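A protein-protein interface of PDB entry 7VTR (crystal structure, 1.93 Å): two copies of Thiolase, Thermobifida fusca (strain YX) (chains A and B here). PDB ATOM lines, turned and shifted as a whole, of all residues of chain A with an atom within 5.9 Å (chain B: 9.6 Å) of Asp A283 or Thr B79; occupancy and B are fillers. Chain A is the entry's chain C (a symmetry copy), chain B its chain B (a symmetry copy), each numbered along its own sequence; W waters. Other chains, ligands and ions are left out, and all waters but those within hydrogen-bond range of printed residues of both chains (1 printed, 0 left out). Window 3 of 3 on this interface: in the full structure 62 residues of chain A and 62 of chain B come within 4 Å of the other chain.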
ATOM      1  N   TRP A 159      26.933  16.297   3.752  1.00  0.00           N
ATOM      2  CA  TRP A 159      26.391  17.425   4.492  1.00  0.00           C
ATOM      3  C   TRP A 159      27.266  18.669   4.416  1.00  0.00           C
ATOM      4  O   TRP A 159      26.779  19.764   4.711  1.00  0.00           O
ATOM      5  CB  TRP A 159      26.139  17.013   5.943  1.00  0.00           C
ATOM      6  CG  TRP A 159      25.086  15.901   6.038  1.00  0.00           C
ATOM      7  CD1 TRP A 159      24.132  15.586   5.105  1.00  0.00           C
ATOM      8  CD2 TRP A 159      24.887  15.002   7.132  1.00  0.00           C
ATOM      9  NE1 TRP A 159      23.367  14.534   5.551  1.00  0.00           N
ATOM     10  CE2 TRP A 159      23.808  14.161   6.795  1.00  0.00           C
ATOM     11  CE3 TRP A 159      25.519  14.829   8.365  1.00  0.00           C
ATOM     12  CZ2 TRP A 159      23.355  13.156   7.640  1.00  0.00           C
ATOM     13  CZ3 TRP A 159      25.066  13.826   9.213  1.00  0.00           C
ATOM     14  CH2 TRP A 159      23.995  13.002   8.848  1.00  0.00           C
ATOM     15  N   ALA A 281      14.735  20.890  11.553  1.00  0.00           N
ATOM     16  CA  ALA A 281      16.010  20.562  10.975  1.00  0.00           C
ATOM     17  C   ALA A 281      15.783  19.474   9.941  1.00  0.00           C
ATOM     18  O   ALA A 281      14.824  18.705  10.021  1.00  0.00           O
ATOM     19  CB  ALA A 281      17.002  20.142  12.045  1.00  0.00           C
ATOM     20  N   VAL A 282      16.648  19.452   8.937  1.00  0.00           N
ATOM     21  CA  VAL A 282      16.514  18.573   7.798  1.00  0.00           C
ATOM     22  C   VAL A 282      17.921  18.121   7.438  1.00  0.00           C
ATOM     23  O   VAL A 282      18.904  18.591   8.027  1.00  0.00           O
ATOM     24  CB  VAL A 282      15.832  19.276   6.602  1.00  0.00           C
ATOM     25  CG1 VAL A 282      14.400  19.672   6.951  1.00  0.00           C
ATOM     26  CG2 VAL A 282      16.624  20.504   6.186  1.00  0.00           C
ATOM     27  N   ASP A 283      18.025  17.191   6.490  1.00  0.00           N
ATOM     28  CA  ASP A 283      19.361  16.841   6.032  1.00  0.00           C
ATOM     29  C   ASP A 283      20.085  18.115   5.630  1.00  0.00           C
ATOM     30  O   ASP A 283      19.507  18.948   4.915  1.00  0.00           O
ATOM     31  CB  ASP A 283      19.362  15.870   4.851  1.00  0.00           C
ATOM     32  CG  ASP A 283      18.917  14.475   5.236  1.00  0.00           C
ATOM     33  OD1 ASP A 283      19.060  14.095   6.425  1.00  0.00           O
ATOM     34  OD2 ASP A 283      18.540  13.711   4.315  1.00  0.00           O
ATOM     35  N   PRO A 284      21.309  18.330   6.105  1.00  0.00           N
ATOM     36  CA  PRO A 284      22.058  19.536   5.721  1.00  0.00           C
ATOM     37  C   PRO A 284      22.079  19.816   4.232  1.00  0.00           C
ATOM     38  O   PRO A 284      22.108  20.985   3.826  1.00  0.00           O
ATOM     39  CB  PRO A 284      23.463  19.231   6.246  1.00  0.00           C
ATOM     40  CG  PRO A 284      23.197  18.437   7.493  1.00  0.00           C
ATOM     41  CD  PRO A 284      22.025  17.540   7.120  1.00  0.00           C
ATOM     42  N   ASP A 285      22.081  18.787   3.393  1.00  0.00           N
ATOM     43  CA  ASP A 285      22.123  19.062   1.965  1.00  0.00           C
ATOM     44  C   ASP A 285      20.778  19.494   1.400  1.00  0.00           C
ATOM     45  O   ASP A 285      20.706  19.825   0.212  1.00  0.00           O
ATOM     46  CB  ASP A 285      22.677  17.848   1.214  1.00  0.00           C
ATOM     47  CG  ASP A 285      21.841  16.607   1.403  1.00  0.00           C
ATOM     48  OD1 ASP A 285      20.961  16.578   2.292  1.00  0.00           O
ATOM     49  OD2 ASP A 285      22.094  15.632   0.664  1.00  0.00           O
ATOM     50  N   VAL A 286      19.724  19.537   2.208  1.00  0.00           N
ATOM     51  CA  VAL A 286      18.474  20.130   1.744  1.00  0.00           C
ATOM     52  C   VAL A 286      18.117  21.284   2.679  1.00  0.00           C
ATOM     53  O   VAL A 286      16.940  21.550   2.942  1.00  0.00           O
ATOM     54  CB  VAL A 286      17.348  19.081   1.652  1.00  0.00           C
ATOM     55  CG1 VAL A 286      17.726  17.966   0.638  1.00  0.00           C
ATOM     56  CG2 VAL A 286      17.050  18.460   3.008  1.00  0.00           C
ATOM     57  N   PHE A 287      19.139  22.002   3.162  1.00  0.00           N
ATOM     58  CA  PHE A 287      18.912  23.055   4.146  1.00  0.00           C
ATOM     59  C   PHE A 287      17.881  24.061   3.664  1.00  0.00           C
ATOM     60  O   PHE A 287      17.108  24.600   4.468  1.00  0.00           O
ATOM     61  CB  PHE A 287      20.222  23.775   4.470  1.00  0.00           C
ATOM     62  CG  PHE A 287      20.580  24.829   3.481  1.00  0.00           C
ATOM     63  CD1 PHE A 287      21.188  24.486   2.283  1.00  0.00           C
ATOM     64  CD2 PHE A 287      20.269  26.158   3.724  1.00  0.00           C
ATOM     65  CE1 PHE A 287      21.512  25.446   1.361  1.00  0.00           C
ATOM     66  CE2 PHE A 287      20.577  27.130   2.787  1.00  0.00           C
ATOM     67  CZ  PHE A 287      21.201  26.768   1.603  1.00  0.00           C
ATOM     68  N   VAL A 381      23.158  24.433   7.759  1.00  0.00           N
ATOM     69  CA  VAL A 381      23.500  23.037   8.006  1.00  0.00           C
ATOM     70  C   VAL A 381      22.250  22.176   8.158  1.00  0.00           C
ATOM     71  O   VAL A 381      22.246  21.176   8.857  1.00  0.00           O
ATOM     72  CB  VAL A 381      24.503  22.880   9.160  1.00  0.00           C
ATOM     73  CG1 VAL A 381      24.994  21.448   9.243  1.00  0.00           C
ATOM     74  CG2 VAL A 381      25.677  23.810   8.920  1.00  0.00           C
ATOM     75  N   GLY A 382      21.178  22.611   7.507  1.00  0.00           N
ATOM     76  CA  GLY A 382      19.927  21.881   7.535  1.00  0.00           C
ATOM     77  C   GLY A 382      18.967  22.296   8.622  1.00  0.00           C
ATOM     78  O   GLY A 382      18.480  21.431   9.345  1.00  0.00           O
ATOM     79  N   PRO B  46      17.095   9.989  20.177  1.00  0.00           N
ATOM     80  CA  PRO B  46      17.592  11.334  19.858  1.00  0.00           C
ATOM     81  C   PRO B  46      16.674  12.139  18.973  1.00  0.00           C
ATOM     82  O   PRO B  46      16.652  13.370  19.093  1.00  0.00           O
ATOM     83  CB  PRO B  46      18.919  11.016  19.151  1.00  0.00           C
ATOM     84  CG  PRO B  46      19.383   9.816  19.904  1.00  0.00           C
ATOM     85  CD  PRO B  46      18.121   8.977  19.878  1.00  0.00           C
ATOM     86  N   ALA B  47      15.931  11.487  18.074  1.00  0.00           N
ATOM     87  CA  ALA B  47      14.949  12.188  17.263  1.00  0.00           C
ATOM     88  C   ALA B  47      13.912  12.916  18.111  1.00  0.00           C
ATOM     89  O   ALA B  47      13.309  13.889  17.642  1.00  0.00           O
ATOM     90  CB  ALA B  47      14.255  11.208  16.321  1.00  0.00           C
ATOM     91  N   VAL B  49      14.605  14.720  20.606  1.00  0.00           N
ATOM     92  CA  VAL B  49      15.195  15.948  21.118  1.00  0.00           C
ATOM     93  C   VAL B  49      14.726  17.081  20.223  1.00  0.00           C
ATOM     94  O   VAL B  49      14.906  17.034  19.003  1.00  0.00           O
ATOM     95  CB  VAL B  49      16.723  15.839  21.164  1.00  0.00           C
ATOM     96  CG1 VAL B  49      17.364  17.174  21.515  1.00  0.00           C
ATOM     97  CG2 VAL B  49      17.115  14.774  22.192  1.00  0.00           C
ATOM     98  N   ASP B  50      14.038  18.059  20.818  1.00  0.00           N
ATOM     99  CA  ASP B  50      13.444  19.125  20.018  1.00  0.00           C
ATOM    100  C   ASP B  50      14.443  20.183  19.629  1.00  0.00           C
ATOM    101  O   ASP B  50      14.236  20.886  18.634  1.00  0.00           O
ATOM    102  CB  ASP B  50      12.292  19.764  20.780  1.00  0.00           C
ATOM    103  CG  ASP B  50      11.180  18.787  21.014  1.00  0.00           C
ATOM    104  OD1 ASP B  50      10.782  18.145  20.014  1.00  0.00           O
ATOM    105  OD2 ASP B  50      10.769  18.603  22.180  1.00  0.00           O
ATOM    106  N   VAL B  52      18.886  21.273  20.405  1.00  0.00           N
ATOM    107  CA  VAL B  52      20.155  21.102  21.100  1.00  0.00           C
ATOM    108  C   VAL B  52      20.769  22.476  21.273  1.00  0.00           C
ATOM    109  O   VAL B  52      21.049  23.166  20.287  1.00  0.00           O
ATOM    110  CB  VAL B  52      21.108  20.175  20.335  1.00  0.00           C
ATOM    111  CG1 VAL B  52      22.451  20.062  21.083  1.00  0.00           C
ATOM    112  CG2 VAL B  52      20.472  18.828  20.197  1.00  0.00           C
ATOM    113  N   ARG B  69      24.599  22.233  16.438  1.00  0.00           N
ATOM    114  CA  ARG B  69      24.135  21.539  15.255  1.00  0.00           C
ATOM    115  C   ARG B  69      25.175  20.554  14.727  1.00  0.00           C
ATOM    116  O   ARG B  69      24.866  19.433  14.419  1.00  0.00           O
ATOM    117  CB  ARG B  69      23.753  22.524  14.167  1.00  0.00           C
ATOM    118  CG  ARG B  69      23.402  21.867  12.859  1.00  0.00           C
ATOM    119  CD  ARG B  69      22.256  20.872  12.990  1.00  0.00           C
ATOM    120  NE  ARG B  69      21.770  20.487  11.676  1.00  0.00           N
ATOM    121  CZ  ARG B  69      20.853  19.561  11.435  1.00  0.00           C
ATOM    122  NH1 ARG B  69      20.278  18.899  12.418  1.00  0.00           N
ATOM    123  NH2 ARG B  69      20.507  19.307  10.197  1.00  0.00           N
ATOM    124  N   MET B  70      26.422  20.986  14.672  1.00  0.00           N
ATOM    125  CA  MET B  70      27.465  20.115  14.212  1.00  0.00           C
ATOM    126  C   MET B  70      27.560  18.917  15.122  1.00  0.00           C
ATOM    127  O   MET B  70      27.703  17.824  14.668  1.00  0.00           O
ATOM    128  CB  MET B  70      28.802  20.805  14.253  1.00  0.00           C
ATOM    129  CG  MET B  70      28.924  22.012  13.377  1.00  0.00           C
ATOM    130  SD  MET B  70      28.314  21.720  11.738  1.00  0.00           S
ATOM    131  CE  MET B  70      28.727  23.266  10.962  1.00  0.00           C
ATOM    132  N   ALA B  72      25.298  17.517  17.045  1.00  0.00           N
ATOM    133  CA  ALA B  72      24.215  16.555  16.867  1.00  0.00           C
ATOM    134  C   ALA B  72      24.487  15.676  15.648  1.00  0.00           C
ATOM    135  O   ALA B  72      24.302  14.452  15.681  1.00  0.00           O
ATOM    136  CB  ALA B  72      22.881  17.294  16.724  1.00  0.00           C
ATOM    137  N   LEU B  73      24.949  16.293  14.565  1.00  0.00           N
ATOM    138  CA  LEU B  73      25.263  15.535  13.358  1.00  0.00           C
ATOM    139  C   LEU B  73      26.418  14.575  13.607  1.00  0.00           C
ATOM    140  O   LEU B  73      26.380  13.407  13.202  1.00  0.00           O
ATOM    141  CB  LEU B  73      25.609  16.501  12.232  1.00  0.00           C
ATOM    142  CG  LEU B  73      24.402  17.331  11.844  1.00  0.00           C
ATOM    143  CD1 LEU B  73      24.796  18.409  10.845  1.00  0.00           C
ATOM    144  CD2 LEU B  73      23.296  16.447  11.291  1.00  0.00           C
ATOM    145  N   LEU B  74      27.458  15.063  14.279  1.00  0.00           N
ATOM    146  CA  LEU B  74      28.621  14.247  14.576  1.00  0.00           C
ATOM    147  C   LEU B  74      28.280  13.130  15.536  1.00  0.00           C
ATOM    148  O   LEU B  74      28.882  12.051  15.466  1.00  0.00           O
ATOM    149  CB  LEU B  74      29.706  15.134  15.161  1.00  0.00           C
ATOM    150  CG  LEU B  74      30.299  16.041  14.100  1.00  0.00           C
ATOM    151  CD1 LEU B  74      31.137  17.109  14.787  1.00  0.00           C
ATOM    152  CD2 LEU B  74      31.138  15.194  13.123  1.00  0.00           C
ATOM    153  N   ALA B  75      27.335  13.375  16.452  1.00  0.00           N
ATOM    154  CA  ALA B  75      26.919  12.353  17.391  1.00  0.00           C
ATOM    155  C   ALA B  75      26.094  11.270  16.731  1.00  0.00           C
ATOM    156  O   ALA B  75      25.715  10.313  17.408  1.00  0.00           O
ATOM    157  CB  ALA B  75      26.128  12.977  18.542  1.00  0.00           C
ATOM    158  N   GLY B  76      25.819  11.402  15.437  1.00  0.00           N
ATOM    159  CA  GLY B  76      24.987  10.445  14.737  1.00  0.00           C
ATOM    160  C   GLY B  76      23.519  10.585  15.030  1.00  0.00           C
ATOM    161  O   GLY B  76      22.770   9.612  14.888  1.00  0.00           O
ATOM    162  N   TRP B  77      23.086  11.767  15.453  1.00  0.00           N
ATOM    163  CA  TRP B  77      21.688  12.008  15.710  1.00  0.00           C
ATOM    164  C   TRP B  77      20.970  12.326  14.417  1.00  0.00           C
ATOM    165  O   TRP B  77      21.596  12.710  13.429  1.00  0.00           O
ATOM    166  CB  TRP B  77      21.511  13.152  16.704  1.00  0.00           C
ATOM    167  CG  TRP B  77      21.915  12.767  18.082  1.00  0.00           C
ATOM    168  CD1 TRP B  77      22.613  11.652  18.445  1.00  0.00           C
ATOM    169  CD2 TRP B  77      21.576  13.443  19.298  1.00  0.00           C
ATOM    170  NE1 TRP B  77      22.761  11.612  19.808  1.00  0.00           N
ATOM    171  CE2 TRP B  77      22.136  12.701  20.355  1.00  0.00           C
ATOM    172  CE3 TRP B  77      20.871  14.613  19.593  1.00  0.00           C
ATOM    173  CZ2 TRP B  77      22.013  13.093  21.690  1.00  0.00           C
ATOM    174  CZ3 TRP B  77      20.752  15.002  20.923  1.00  0.00           C
ATOM    175  CH2 TRP B  77      21.321  14.247  21.949  1.00  0.00           C
ATOM    176  N   PRO B  78      19.655  12.136  14.383  1.00  0.00           N
ATOM    177  CA  PRO B  78      18.919  12.430  13.155  1.00  0.00           C
ATOM    178  C   PRO B  78      19.151  13.875  12.767  1.00  0.00           C
ATOM    179  O   PRO B  78      19.271  14.757  13.622  1.00  0.00           O
ATOM    180  CB  PRO B  78      17.461  12.172  13.539  1.00  0.00           C
ATOM    181  CG  PRO B  78      17.570  11.119  14.606  1.00  0.00           C
ATOM    182  CD  PRO B  78      18.797  11.518  15.406  1.00  0.00           C
ATOM    183  N   THR B  79      19.242  14.103  11.465  1.00  0.00           N
ATOM    184  CA  THR B  79      19.375  15.460  10.982  1.00  0.00           C
ATOM    185  C   THR B  79      18.164  16.302  11.322  1.00  0.00           C
ATOM    186  O   THR B  79      18.201  17.513  11.109  1.00  0.00           O
ATOM    187  CB  THR B  79      19.542  15.466   9.477  1.00  0.00           C
ATOM    188  OG1 THR B  79      18.415  14.802   8.897  1.00  0.00           O
ATOM    189  CG2 THR B  79      20.821  14.736   9.082  1.00  0.00           C
ATOM    190  N   SER B  80      17.081  15.686  11.787  1.00  0.00           N
ATOM    191  CA  SER B  80      15.907  16.439  12.192  1.00  0.00           C
ATOM    192  C   SER B  80      16.094  17.131  13.537  1.00  0.00           C
ATOM    193  O   SER B  80      15.221  17.905  13.940  1.00  0.00           O
ATOM    194  CB  SER B  80      14.706  15.512  12.286  1.00  0.00           C
ATOM    195  OG  SER B  80      15.010  14.485  13.196  1.00  0.00           O
ATOM    196  N   VAL B  81      17.191  16.868  14.239  1.00  0.00           N
ATOM    197  CA  VAL B  81      17.415  17.503  15.536  1.00  0.00           C
ATOM    198  C   VAL B  81      18.084  18.854  15.337  1.00  0.00           C
ATOM    199  O   VAL B  81      19.231  18.927  14.858  1.00  0.00           O
ATOM    200  CB  VAL B  81      18.237  16.601  16.458  1.00  0.00           C
ATOM    201  CG1 VAL B  81      18.400  17.258  17.839  1.00  0.00           C
ATOM    202  CG2 VAL B  81      17.536  15.264  16.576  1.00  0.00           C
ATOM    203  N   PRO B  82      17.403  19.941  15.676  1.00  0.00           N
ATOM    204  CA  PRO B  82      18.004  21.259  15.522  1.00  0.00           C
ATOM    205  C   PRO B  82      19.036  21.512  16.605  1.00  0.00           C
ATOM    206  O   PRO B  82      19.082  20.858  17.649  1.00  0.00           O
ATOM    207  CB  PRO B  82      16.817  22.226  15.657  1.00  0.00           C
ATOM    208  CG  PRO B  82      15.594  21.386  15.756  1.00  0.00           C
ATOM    209  CD  PRO B  82      16.052  20.031  16.232  1.00  0.00           C
ATOM    210  N   GLY B  83      19.888  22.473  16.320  1.00  0.00           N
ATOM    211  CA  GLY B  83      20.867  22.878  17.291  1.00  0.00           C
ATOM    212  C   GLY B  83      21.150  24.352  17.170  1.00  0.00           C
ATOM    213  O   GLY B  83      21.141  24.939  16.083  1.00  0.00           O
HETATM  214  O   HOH W   1      13.090  18.959  13.044  1.00  0.00           O
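No position is printed for both chains.
Of the 17 pairs that touch across the chains among the printed residues, none has its exchanged pair printed and touching as well.
The guanidinium group (NH2) of Arg B69 lies within hydrogen-bond range of the backbone carbonyl oxygen (O) of Val A282 (2.8 Å).
O of Val A381 lies within hydrogen-bond range of NH2 of Arg B69 (2.9 Å).
The backbone carbonyl oxygen (O) of Gly A382 lies within hydrogen-bond range of the guanidinium group (NH2) of Arg B69 (3.1 Å).
The backbone carbonyl oxygen of Thr B79 lies within hydrogen-bond range of the backbone NH of Val A282 (3.3 Å).
The side-chain hydroxyl (OG1) of Thr B79 lies within hydrogen-bond range of the side-chain carboxylate (OD1) of Asp A283.
Thr B79 touches just these residues of chain A: Trp A159 (3.3 Å), Ala A281 (3.0 Å), Val A282 (3.3 Å), Asp A283 (2.7 Å) and Pro A284 (3.6 Å).
Ala A281 touches five residues of chain B.
Of chain B, only Arg B69 (2.8 Å) and Thr B79 (3.3 Å) come within 4 Å of Val A282.
Of chain B, only Arg B69 (3.9 Å), Leu B73 (3.7 Å) and Thr B79 (3.6 Å) come within 4 Å of Pro A284.
No residue of chain B comes within 4 Å of Asp A285.
Val A286 touches none of the printed residues of chain B.
Gly A382 touches just one residue of chain B: Arg B69.
Printed residues of chain A within 4 Å of Val B81: Ala A281 (3.7 Å).
Printed residues of chain B within 4 Å of Trp A159: Leu B73 and Thr B79.
Of the printed residues of chain A, Leu B73 touches Trp A159 (3.8 Å), Pro A284 (3.7 Å) and Val A381 (3.4 Å).
Of the printed residues of chain A, Met B70 touches Val A381 (3.7 Å).
Gly B76 touches none of the printed residues of chain A.
Asp B50 touches none of the printed residues of chain A.
The nearest residue of chain A that does not touch Thr B79 is Gly A382 (4.3 Å).
Water W1 bridges the backbone carbonyl oxygen (O) of Ser B80 (2.5 Å) and the backbone NH (N) of Ala A281 (2.9 Å).
The backbone carbonyl oxygen (O) of Pro B82 sits at hydrogen-bond distance from the backbone NH (N) of Val B52 (2.8 Å).
The guanidinium group of Arg B69 is in hydrogen-bond range of the backbone carbonyl oxygen of Thr B79 (2.8 Å).
O of Val B81 lies within hydrogen-bond range of NH1 of Arg B69 (2.7 Å).
The backbone NH of Val A282 sits at hydrogen-bond distance from the backbone carbonyl oxygen of Gly A382, at 2.7 Å.
Trp A159 touches Leu B73.
CZ2 of Trp A159 touches CG2 of Thr B79, 3.3 Å away.
Ala A281 touches Arg B69 (CB to NH1, 3.5 Å).
CA of Ser B80 touches O of Ala A281, at 3.3 Å.
CB of Ala A281 touches C of Val B81 (3.7 Å).
Ala A281 touches Pro B82 (CB to N, 3.7 Å).
CD of Pro A284 touches NH2 of Arg B69, at 3.9 Å.
CG2 of Thr B79 touches CD of Pro A284 (3.6 Å).
Val A381 touches Met B70.
Leu B73 touches Val A381.
Of the 19 printed residues of chain B, 7 touch a printed residue of chain A.
Printed residues of chain A that touch a printed residue of chain B: Trp A159, Ala A281, Val A282, Asp A283, Pro A284, Val A381 and Gly A382.
Along chain A the printed residues that touch a printed residue of chain B span positions 159 to 382.
Among the printed residues, no Asp or Glu carboxylate lies within 4 Å of a Lys or Arg side-chain nitrogen of the other chain.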
